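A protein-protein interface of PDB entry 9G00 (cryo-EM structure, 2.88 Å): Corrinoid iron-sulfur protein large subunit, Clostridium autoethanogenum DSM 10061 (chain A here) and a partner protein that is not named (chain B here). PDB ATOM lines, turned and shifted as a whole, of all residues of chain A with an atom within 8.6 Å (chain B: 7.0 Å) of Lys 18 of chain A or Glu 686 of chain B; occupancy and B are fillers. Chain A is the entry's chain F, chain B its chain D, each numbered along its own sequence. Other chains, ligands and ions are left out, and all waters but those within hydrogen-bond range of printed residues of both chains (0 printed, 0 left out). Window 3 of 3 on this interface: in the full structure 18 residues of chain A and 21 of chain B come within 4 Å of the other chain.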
ATOM      1  N   LYS A  15      -7.489 -15.739  32.283  1.00  0.00           N
ATOM      2  CA  LYS A  15      -8.360 -16.044  33.407  1.00  0.00           C
ATOM      3  C   LYS A  15      -9.215 -17.283  33.189  1.00  0.00           C
ATOM      4  O   LYS A  15      -9.742 -17.825  34.164  1.00  0.00           O
ATOM      5  CB  LYS A  15      -9.282 -14.850  33.700  1.00  0.00           C
ATOM      6  CG  LYS A  15      -8.543 -13.530  33.896  1.00  0.00           C
ATOM      7  CD  LYS A  15      -7.732 -13.515  35.184  1.00  0.00           C
ATOM      8  CE  LYS A  15      -7.101 -12.150  35.450  1.00  0.00           C
ATOM      9  NZ  LYS A  15      -5.893 -11.894  34.614  1.00  0.00           N
ATOM     10  N   ASN A  16      -9.364 -17.739  31.948  1.00  0.00           N
ATOM     11  CA  ASN A  16     -10.158 -18.925  31.635  1.00  0.00           C
ATOM     12  C   ASN A  16     -11.556 -18.822  32.244  1.00  0.00           C
ATOM     13  O   ASN A  16     -12.086 -19.780  32.809  1.00  0.00           O
ATOM     14  CB  ASN A  16      -9.453 -20.195  32.114  1.00  0.00           C
ATOM     15  CG  ASN A  16      -8.026 -20.302  31.606  1.00  0.00           C
ATOM     16  OD1 ASN A  16      -7.621 -19.580  30.695  1.00  0.00           O
ATOM     17  ND2 ASN A  16      -7.255 -21.210  32.194  1.00  0.00           N
ATOM     18  N   CYS A  17     -12.156 -17.641  32.126  1.00  0.00           N
ATOM     19  CA  CYS A  17     -13.456 -17.355  32.716  1.00  0.00           C
ATOM     20  C   CYS A  17     -14.620 -17.653  31.779  1.00  0.00           C
ATOM     21  O   CYS A  17     -15.774 -17.550  32.198  1.00  0.00           O
ATOM     22  CB  CYS A  17     -13.529 -15.898  33.175  1.00  0.00           C
ATOM     23  SG  CYS A  17     -13.196 -14.689  31.905  1.00  0.00           S
ATOM     24  N   LYS A  18     -14.347 -18.030  30.529  1.00  0.00           N
ATOM     25  CA  LYS A  18     -15.388 -18.409  29.575  1.00  0.00           C
ATOM     26  C   LYS A  18     -16.359 -17.269  29.270  1.00  0.00           C
ATOM     27  O   LYS A  18     -17.485 -17.513  28.829  1.00  0.00           O
ATOM     28  CB  LYS A  18     -16.094 -19.680  30.060  1.00  0.00           C
ATOM     29  CG  LYS A  18     -15.128 -20.826  30.286  1.00  0.00           C
ATOM     30  CD  LYS A  18     -15.657 -22.008  31.039  1.00  0.00           C
ATOM     31  CE  LYS A  18     -14.620 -23.108  31.102  1.00  0.00           C
ATOM     32  NZ  LYS A  18     -15.144 -24.327  31.760  1.00  0.00           N
ATOM     33  N   ASP A  19     -15.931 -16.013  29.447  1.00  0.00           N
ATOM     34  CA  ASP A  19     -16.811 -14.877  29.177  1.00  0.00           C
ATOM     35  C   ASP A  19     -16.983 -14.684  27.662  1.00  0.00           C
ATOM     36  O   ASP A  19     -18.067 -14.289  27.219  1.00  0.00           O
ATOM     37  CB  ASP A  19     -16.344 -13.597  29.895  1.00  0.00           C
ATOM     38  CG  ASP A  19     -16.543 -13.642  31.413  1.00  0.00           C
ATOM     39  OD1 ASP A  19     -16.835 -14.724  31.967  1.00  0.00           O
ATOM     40  OD2 ASP A  19     -16.415 -12.577  32.050  1.00  0.00           O
ATOM     41  N   CYS A  20     -15.959 -15.009  26.849  1.00  0.00           N
ATOM     42  CA  CYS A  20     -16.003 -14.865  25.385  1.00  0.00           C
ATOM     43  C   CYS A  20     -16.790 -15.978  24.738  1.00  0.00           C
ATOM     44  O   CYS A  20     -16.933 -15.977  23.512  1.00  0.00           O
ATOM     45  CB  CYS A  20     -14.631 -14.939  24.694  1.00  0.00           C
ATOM     46  SG  CYS A  20     -13.570 -16.260  25.290  1.00  0.00           S
ATOM     47  N   GLY A  21     -17.260 -16.935  25.514  1.00  0.00           N
ATOM     48  CA  GLY A  21     -17.959 -18.041  24.927  1.00  0.00           C
ATOM     49  C   GLY A  21     -17.083 -19.222  24.589  1.00  0.00           C
ATOM     50  O   GLY A  21     -17.608 -20.264  24.182  1.00  0.00           O
ATOM     51  N   PHE A  22     -15.759 -19.090  24.727  1.00  0.00           N
ATOM     52  CA  PHE A  22     -14.852 -20.201  24.507  1.00  0.00           C
ATOM     53  C   PHE A  22     -14.261 -20.671  25.840  1.00  0.00           C
ATOM     54  O   PHE A  22     -14.092 -19.873  26.765  1.00  0.00           O
ATOM     55  CB  PHE A  22     -13.711 -19.807  23.560  1.00  0.00           C
ATOM     56  CG  PHE A  22     -14.117 -19.729  22.112  1.00  0.00           C
ATOM     57  CD1 PHE A  22     -15.406 -20.043  21.708  1.00  0.00           C
ATOM     58  CD2 PHE A  22     -13.197 -19.353  21.148  1.00  0.00           C
ATOM     59  CE1 PHE A  22     -15.767 -19.976  20.379  1.00  0.00           C
ATOM     60  CE2 PHE A  22     -13.557 -19.285  19.817  1.00  0.00           C
ATOM     61  CZ  PHE A  22     -14.842 -19.599  19.434  1.00  0.00           C
ATOM     62  N   PRO A  23     -13.944 -21.968  25.960  1.00  0.00           N
ATOM     63  CA  PRO A  23     -13.515 -22.481  27.280  1.00  0.00           C
ATOM     64  C   PRO A  23     -12.288 -21.795  27.847  1.00  0.00           C
ATOM     65  O   PRO A  23     -12.336 -21.291  28.974  1.00  0.00           O
ATOM     66  CB  PRO A  23     -13.259 -23.971  26.995  1.00  0.00           C
ATOM     67  CG  PRO A  23     -14.103 -24.284  25.811  1.00  0.00           C
ATOM     68  CD  PRO A  23     -14.069 -23.046  24.969  1.00  0.00           C
ATOM     69  N   THR A  24     -11.184 -21.762  27.107  1.00  0.00           N
ATOM     70  CA  THR A  24      -9.933 -21.227  27.613  1.00  0.00           C
ATOM     71  C   THR A  24      -9.548 -19.965  26.854  1.00  0.00           C
ATOM     72  O   THR A  24     -10.010 -19.714  25.737  1.00  0.00           O
ATOM     73  CB  THR A  24      -8.802 -22.257  27.509  1.00  0.00           C
ATOM     74  OG1 THR A  24      -8.524 -22.536  26.132  1.00  0.00           O
ATOM     75  CG2 THR A  24      -9.187 -23.546  28.226  1.00  0.00           C
ATOM     76  N   CYS A  25      -8.687 -19.165  27.486  1.00  0.00           N
ATOM     77  CA  CYS A  25      -8.143 -17.997  26.808  1.00  0.00           C
ATOM     78  C   CYS A  25      -7.343 -18.401  25.578  1.00  0.00           C
ATOM     79  O   CYS A  25      -7.343 -17.695  24.566  1.00  0.00           O
ATOM     80  CB  CYS A  25      -7.262 -17.202  27.771  1.00  0.00           C
ATOM     81  SG  CYS A  25      -8.137 -16.405  29.125  1.00  0.00           S
ATOM     82  N   PHE A  28      -9.754 -18.984  22.842  1.00  0.00           N
ATOM     83  CA  PHE A  28     -10.075 -17.664  22.316  1.00  0.00           C
ATOM     84  C   PHE A  28      -8.886 -17.026  21.613  1.00  0.00           C
ATOM     85  O   PHE A  28      -9.081 -16.171  20.745  1.00  0.00           O
ATOM     86  CB  PHE A  28     -10.561 -16.763  23.453  1.00  0.00           C
ATOM     87  CG  PHE A  28     -10.908 -15.366  23.021  1.00  0.00           C
ATOM     88  CD1 PHE A  28     -12.124 -15.093  22.424  1.00  0.00           C
ATOM     89  CD2 PHE A  28     -10.019 -14.323  23.224  1.00  0.00           C
ATOM     90  CE1 PHE A  28     -12.444 -13.809  22.030  1.00  0.00           C
ATOM     91  CE2 PHE A  28     -10.336 -13.038  22.831  1.00  0.00           C
ATOM     92  CZ  PHE A  28     -11.548 -12.782  22.235  1.00  0.00           C
ATOM     93  N   LYS A  41     -15.706 -10.319  21.990  1.00  0.00           N
ATOM     94  CA  LYS A  41     -16.331 -11.231  22.937  1.00  0.00           C
ATOM     95  C   LYS A  41     -15.707 -11.159  24.324  1.00  0.00           C
ATOM     96  O   LYS A  41     -16.346 -11.573  25.296  1.00  0.00           O
ATOM     97  CB  LYS A  41     -16.257 -12.667  22.417  1.00  0.00           C
ATOM     98  CG  LYS A  41     -17.289 -13.009  21.353  1.00  0.00           C
ATOM     99  CD  LYS A  41     -16.868 -12.553  19.964  1.00  0.00           C
ATOM    100  CE  LYS A  41     -17.557 -11.262  19.549  1.00  0.00           C
ATOM    101  NZ  LYS A  41     -17.104 -10.808  18.204  1.00  0.00           N
ATOM    102  N   CYS A  42     -14.486 -10.638  24.446  1.00  0.00           N
ATOM    103  CA  CYS A  42     -13.800 -10.625  25.729  1.00  0.00           C
ATOM    104  C   CYS A  42     -13.973  -9.266  26.391  1.00  0.00           C
ATOM    105  O   CYS A  42     -13.408  -8.276  25.900  1.00  0.00           O
ATOM    106  CB  CYS A  42     -12.319 -10.941  25.550  1.00  0.00           C
ATOM    107  SG  CYS A  42     -11.434 -11.167  27.112  1.00  0.00           S
ATOM    108  N   PRO A  43     -14.731  -9.156  27.493  1.00  0.00           N
ATOM    109  CA  PRO A  43     -14.890  -7.847  28.141  1.00  0.00           C
ATOM    110  C   PRO A  43     -13.772  -7.531  29.122  1.00  0.00           C
ATOM    111  O   PRO A  43     -13.526  -6.362  29.435  1.00  0.00           O
ATOM    112  CB  PRO A  43     -16.241  -7.973  28.866  1.00  0.00           C
ATOM    113  CG  PRO A  43     -16.800  -9.336  28.486  1.00  0.00           C
ATOM    114  CD  PRO A  43     -15.627 -10.157  28.092  1.00  0.00           C
ATOM    115  N   HIS A  44     -13.076  -8.562  29.598  1.00  0.00           N
ATOM    116  CA  HIS A  44     -12.062  -8.394  30.631  1.00  0.00           C
ATOM    117  C   HIS A  44     -10.732  -7.892  30.087  1.00  0.00           C
ATOM    118  O   HIS A  44      -9.784  -7.737  30.864  1.00  0.00           O
ATOM    119  CB  HIS A  44     -11.849  -9.718  31.370  1.00  0.00           C
ATOM    120  CG  HIS A  44     -13.039 -10.166  32.160  1.00  0.00           C
ATOM    121  ND1 HIS A  44     -14.182  -9.404  32.280  1.00  0.00           N
ATOM    122  CD2 HIS A  44     -13.265 -11.295  32.872  1.00  0.00           C
ATOM    123  CE1 HIS A  44     -15.060 -10.044  33.031  1.00  0.00           C
ATOM    124  NE2 HIS A  44     -14.528 -11.194  33.403  1.00  0.00           N
ATOM    125  N   MET B 584       0.286 -25.636  26.736  1.00  0.00           N
ATOM    126  CA  MET B 584      -0.656 -25.277  27.797  1.00  0.00           C
ATOM    127  C   MET B 584       0.066 -24.325  28.742  1.00  0.00           C
ATOM    128  O   MET B 584       0.714 -24.763  29.703  1.00  0.00           O
ATOM    129  CB  MET B 584      -1.159 -26.513  28.531  1.00  0.00           C
ATOM    130  CG  MET B 584      -2.127 -26.199  29.643  1.00  0.00           C
ATOM    131  SD  MET B 584      -2.885 -27.669  30.347  1.00  0.00           S
ATOM    132  CE  MET B 584      -3.764 -26.944  31.723  1.00  0.00           C
ATOM    133  N   GLU B 586      -0.673 -22.342  31.245  1.00  0.00           N
ATOM    134  CA  GLU B 586      -0.937 -22.309  32.679  1.00  0.00           C
ATOM    135  C   GLU B 586      -0.322 -23.493  33.413  1.00  0.00           C
ATOM    136  O   GLU B 586      -0.159 -23.426  34.635  1.00  0.00           O
ATOM    137  CB  GLU B 586      -2.444 -22.265  32.953  1.00  0.00           C
ATOM    138  CG  GLU B 586      -3.236 -23.468  32.453  1.00  0.00           C
ATOM    139  CD  GLU B 586      -3.678 -23.321  31.015  1.00  0.00           C
ATOM    140  OE1 GLU B 586      -3.111 -22.466  30.304  1.00  0.00           O
ATOM    141  OE2 GLU B 586      -4.595 -24.054  30.596  1.00  0.00           O
ATOM    142  N   THR B 600     -12.838 -33.414  24.296  1.00  0.00           N
ATOM    143  CA  THR B 600     -12.223 -32.097  24.379  1.00  0.00           C
ATOM    144  C   THR B 600     -10.970 -32.165  25.240  1.00  0.00           C
ATOM    145  O   THR B 600     -10.987 -32.742  26.331  1.00  0.00           O
ATOM    146  CB  THR B 600     -13.203 -31.078  24.965  1.00  0.00           C
ATOM    147  OG1 THR B 600     -14.393 -31.040  24.167  1.00  0.00           O
ATOM    148  CG2 THR B 600     -12.582 -29.684  25.007  1.00  0.00           C
ATOM    149  N   THR B 601      -9.885 -31.585  24.737  1.00  0.00           N
ATOM    150  CA  THR B 601      -8.637 -31.506  25.472  1.00  0.00           C
ATOM    151  C   THR B 601      -8.714 -30.404  26.523  1.00  0.00           C
ATOM    152  O   THR B 601      -9.585 -29.536  26.465  1.00  0.00           O
ATOM    153  CB  THR B 601      -7.472 -31.233  24.526  1.00  0.00           C
ATOM    154  OG1 THR B 601      -7.654 -29.966  23.885  1.00  0.00           O
ATOM    155  CG2 THR B 601      -7.376 -32.316  23.473  1.00  0.00           C
ATOM    156  N   PRO B 602      -7.809 -30.419  27.502  1.00  0.00           N
ATOM    157  CA  PRO B 602      -7.772 -29.313  28.469  1.00  0.00           C
ATOM    158  C   PRO B 602      -7.528 -27.964  27.829  1.00  0.00           C
ATOM    159  O   PRO B 602      -7.815 -26.938  28.457  1.00  0.00           O
ATOM    160  CB  PRO B 602      -6.623 -29.707  29.404  1.00  0.00           C
ATOM    161  CG  PRO B 602      -6.567 -31.181  29.317  1.00  0.00           C
ATOM    162  CD  PRO B 602      -6.918 -31.520  27.900  1.00  0.00           C
ATOM    163  N   LEU B 603      -6.990 -27.925  26.610  1.00  0.00           N
ATOM    164  CA  LEU B 603      -6.832 -26.664  25.896  1.00  0.00           C
ATOM    165  C   LEU B 603      -8.163 -26.051  25.482  1.00  0.00           C
ATOM    166  O   LEU B 603      -8.184 -24.885  25.076  1.00  0.00           O
ATOM    167  CB  LEU B 603      -5.961 -26.869  24.656  1.00  0.00           C
ATOM    168  CG  LEU B 603      -4.540 -27.385  24.890  1.00  0.00           C
ATOM    169  CD1 LEU B 603      -3.836 -27.561  23.564  1.00  0.00           C
ATOM    170  CD2 LEU B 603      -3.751 -26.450  25.791  1.00  0.00           C
ATOM    171  N   GLY B 604      -9.263 -26.793  25.577  1.00  0.00           N
ATOM    172  CA  GLY B 604     -10.552 -26.313  25.132  1.00  0.00           C
ATOM    173  C   GLY B 604     -10.865 -26.596  23.680  1.00  0.00           C
ATOM    174  O   GLY B 604     -11.950 -26.226  23.214  1.00  0.00           O
ATOM    175  N   TRP B 648      -0.520 -33.913  29.834  1.00  0.00           N
ATOM    176  CA  TRP B 648      -1.856 -34.475  29.646  1.00  0.00           C
ATOM    177  C   TRP B 648      -1.871 -35.257  28.340  1.00  0.00           C
ATOM    178  O   TRP B 648      -1.536 -34.707  27.290  1.00  0.00           O
ATOM    179  CB  TRP B 648      -2.913 -33.373  29.629  1.00  0.00           C
ATOM    180  CG  TRP B 648      -4.324 -33.860  29.731  1.00  0.00           C
ATOM    181  CD1 TRP B 648      -5.087 -33.907  30.855  1.00  0.00           C
ATOM    182  CD2 TRP B 648      -5.148 -34.354  28.666  1.00  0.00           C
ATOM    183  NE1 TRP B 648      -6.332 -34.403  30.564  1.00  0.00           N
ATOM    184  CE2 TRP B 648      -6.396 -34.685  29.226  1.00  0.00           C
ATOM    185  CE3 TRP B 648      -4.952 -34.549  27.296  1.00  0.00           C
ATOM    186  CZ2 TRP B 648      -7.441 -35.200  28.466  1.00  0.00           C
ATOM    187  CZ3 TRP B 648      -5.992 -35.063  26.544  1.00  0.00           C
ATOM    188  CH2 TRP B 648      -7.219 -35.381  27.131  1.00  0.00           C
ATOM    189  N   CYS B 679      -1.208 -36.720  33.592  1.00  0.00           N
ATOM    190  CA  CYS B 679      -2.654 -36.765  33.717  1.00  0.00           C
ATOM    191  C   CYS B 679      -3.283 -37.333  32.451  1.00  0.00           C
ATOM    192  O   CYS B 679      -2.710 -37.265  31.362  1.00  0.00           O
ATOM    193  CB  CYS B 679      -3.203 -35.368  33.988  1.00  0.00           C
ATOM    194  SG  CYS B 679      -4.992 -35.312  34.117  1.00  0.00           S
ATOM    195  N   ALA B 684      -9.056 -36.109  34.824  1.00  0.00           N
ATOM    196  CA  ALA B 684      -9.624 -34.776  34.686  1.00  0.00           C
ATOM    197  C   ALA B 684      -9.629 -34.390  33.214  1.00  0.00           C
ATOM    198  O   ALA B 684      -9.002 -35.041  32.375  1.00  0.00           O
ATOM    199  CB  ALA B 684      -8.850 -33.751  35.521  1.00  0.00           C
ATOM    200  N   THR B 685     -10.368 -33.323  32.913  1.00  0.00           N
ATOM    201  CA  THR B 685     -10.438 -32.779  31.562  1.00  0.00           C
ATOM    202  C   THR B 685     -10.319 -31.264  31.510  1.00  0.00           C
ATOM    203  O   THR B 685     -10.091 -30.727  30.423  1.00  0.00           O
ATOM    204  CB  THR B 685     -11.754 -33.190  30.886  1.00  0.00           C
ATOM    205  OG1 THR B 685     -12.023 -34.571  31.159  1.00  0.00           O
ATOM    206  CG2 THR B 685     -11.676 -32.991  29.381  1.00  0.00           C
ATOM    207  N   GLU B 686     -10.460 -30.556  32.627  1.00  0.00           N
ATOM    208  CA  GLU B 686     -10.414 -29.104  32.655  1.00  0.00           C
ATOM    209  C   GLU B 686      -9.042 -28.618  33.105  1.00  0.00           C
ATOM    210  O   GLU B 686      -8.312 -29.311  33.816  1.00  0.00           O
ATOM    211  CB  GLU B 686     -11.498 -28.554  33.584  1.00  0.00           C
ATOM    212  CG  GLU B 686     -12.907 -28.979  33.198  1.00  0.00           C
ATOM    213  CD  GLU B 686     -13.307 -28.490  31.818  1.00  0.00           C
ATOM    214  OE1 GLU B 686     -12.801 -27.430  31.393  1.00  0.00           O
ATOM    215  OE2 GLU B 686     -14.123 -29.165  31.156  1.00  0.00           O
ATOM    216  N   SER B 687      -8.706 -27.393  32.696  1.00  0.00           N
ATOM    217  CA  SER B 687      -7.366 -26.873  32.950  1.00  0.00           C
ATOM    218  C   SER B 687      -7.095 -26.720  34.441  1.00  0.00           C
ATOM    219  O   SER B 687      -6.015 -27.083  34.919  1.00  0.00           O
ATOM    220  CB  SER B 687      -7.172 -25.538  32.232  1.00  0.00           C
ATOM    221  OG  SER B 687      -8.012 -24.535  32.775  1.00  0.00           O
ATOM    222  N   GLU B 688      -8.058 -26.192  35.200  1.00  0.00           N
ATOM    223  CA  GLU B 688      -7.794 -25.945  36.615  1.00  0.00           C
ATOM    224  C   GLU B 688      -7.697 -27.249  37.397  1.00  0.00           C
ATOM    225  O   GLU B 688      -7.005 -27.302  38.420  1.00  0.00           O
ATOM    226  CB  GLU B 688      -8.867 -25.022  37.206  1.00  0.00           C
ATOM    227  CG  GLU B 688      -9.996 -25.695  37.993  1.00  0.00           C
ATOM    228  CD  GLU B 688     -10.993 -26.410  37.103  1.00  0.00           C
ATOM    229  OE1 GLU B 688     -10.774 -26.454  35.875  1.00  0.00           O
ATOM    230  OE2 GLU B 688     -12.001 -26.922  37.633  1.00  0.00           O
ATOM    231  N   GLU B 689      -8.375 -28.303  36.942  1.00  0.00           N
ATOM    232  CA  GLU B 689      -8.297 -29.581  37.640  1.00  0.00           C
ATOM    233  C   GLU B 689      -6.949 -30.251  37.408  1.00  0.00           C
ATOM    234  O   GLU B 689      -6.339 -30.774  38.347  1.00  0.00           O
ATOM    235  CB  GLU B 689      -9.431 -30.499  37.190  1.00  0.00           C
ATOM    236  CG  GLU B 689     -10.818 -29.954  37.467  1.00  0.00           C
ATOM    237  CD  GLU B 689     -11.912 -30.893  37.004  1.00  0.00           C
ATOM    238  OE1 GLU B 689     -11.585 -32.006  36.540  1.00  0.00           O
ATOM    239  OE2 GLU B 689     -13.100 -30.519  37.102  1.00  0.00           O
ATOM    240  N   VAL B 690      -6.466 -30.243  36.164  1.00  0.00           N
ATOM    241  CA  VAL B 690      -5.214 -30.928  35.866  1.00  0.00           C
ATOM    242  C   VAL B 690      -4.042 -30.216  36.529  1.00  0.00           C
ATOM    243  O   VAL B 690      -3.091 -30.866  36.977  1.00  0.00           O
ATOM    244  CB  VAL B 690      -5.022 -31.052  34.342  1.00  0.00           C
ATOM    245  CG1 VAL B 690      -6.225 -31.738  33.716  1.00  0.00           C
ATOM    246  CG2 VAL B 690      -4.823 -29.702  33.708  1.00  0.00           C
ATOM    247  N   VAL B 691      -4.089 -28.886  36.623  1.00  0.00           N
ATOM    248  CA  VAL B 691      -3.012 -28.162  37.295  1.00  0.00           C
ATOM    249  C   VAL B 691      -2.918 -28.594  38.752  1.00  0.00           C
ATOM    250  O   VAL B 691      -1.821 -28.810  39.279  1.00  0.00           O
ATOM    251  CB  VAL B 691      -3.220 -26.642  37.165  1.00  0.00           C
ATOM    252  CG1 VAL B 691      -2.233 -25.879  38.048  1.00  0.00           C
ATOM    253  CG2 VAL B 691      -3.061 -26.214  35.717  1.00  0.00           C
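The side-chain amino group (NZ) of Lys 18 of chain A is in salt-bridge range of the side-chain carboxylate (OE1) of Glu 686 of chain B (3.9 Å).
The side-chain hydroxyl (OG1) of Thr 24 of chain A lies within hydrogen-bond range of the backbone carbonyl oxygen (O) of Leu 603 of chain B (2.6 Å).
The side-chain amide nitrogen (ND2) of Asn 16 of chain A sits at hydrogen-bond distance from the side-chain hydroxyl (OG) of Ser 687 of chain B, at 3.5 Å.
Among the printed residues, merely in contact across the chains: Pro 23 of chain A with Gly 604 of chain B (3.9 Å) and Thr 24 of chain A with Pro 602 of chain B (3.7 Å).
The backbone NH of Cys 25 of chain A lies within hydrogen-bond range of the side-chain amide oxygen of Asn 16 of chain A (3.4 Å).
The backbone NH (N) of Leu 603 of chain B lies close to the side-chain hydroxyl (OG1) of Thr 601 of chain B, 3.5 Å away.
Of the 17 printed residues of chain B, 5 touch a printed residue of chain A.
Of the 16 printed residues of chain A, 4 touch a printed residue of chain B.
Along chain A the printed residues that touch a printed residue of chain B span positions 16 to 24.
Among the printed residues, 5 pairs touch across the chains.
Among the printed residues, Asp or Glu carboxylates within 4 Å of a Lys or Arg side-chain nitrogen of the other chain: Lys 18 of chain A with Glu 686 of chain B (3.9 Å).
Of chain A, only Lys 18 (3.9 Å) comes within 4 Å of Glu 686 of chain B.
Of chain A, only Asn 16 (3.5 Å) comes within 4 Å of Ser 687 of chain B.
Printed residues of chain B within 4 Å of Asn 16 of chain A: Ser 687 (3.5 Å).
Of the printed residues of chain B, Pro 23 of chain A touches Gly 604.
Printed residues of chain A within 4 Å of Gly 604 of chain B: Pro 23 (3.9 Å).
Gly 21 of chain A touches none of the printed residues of chain B.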
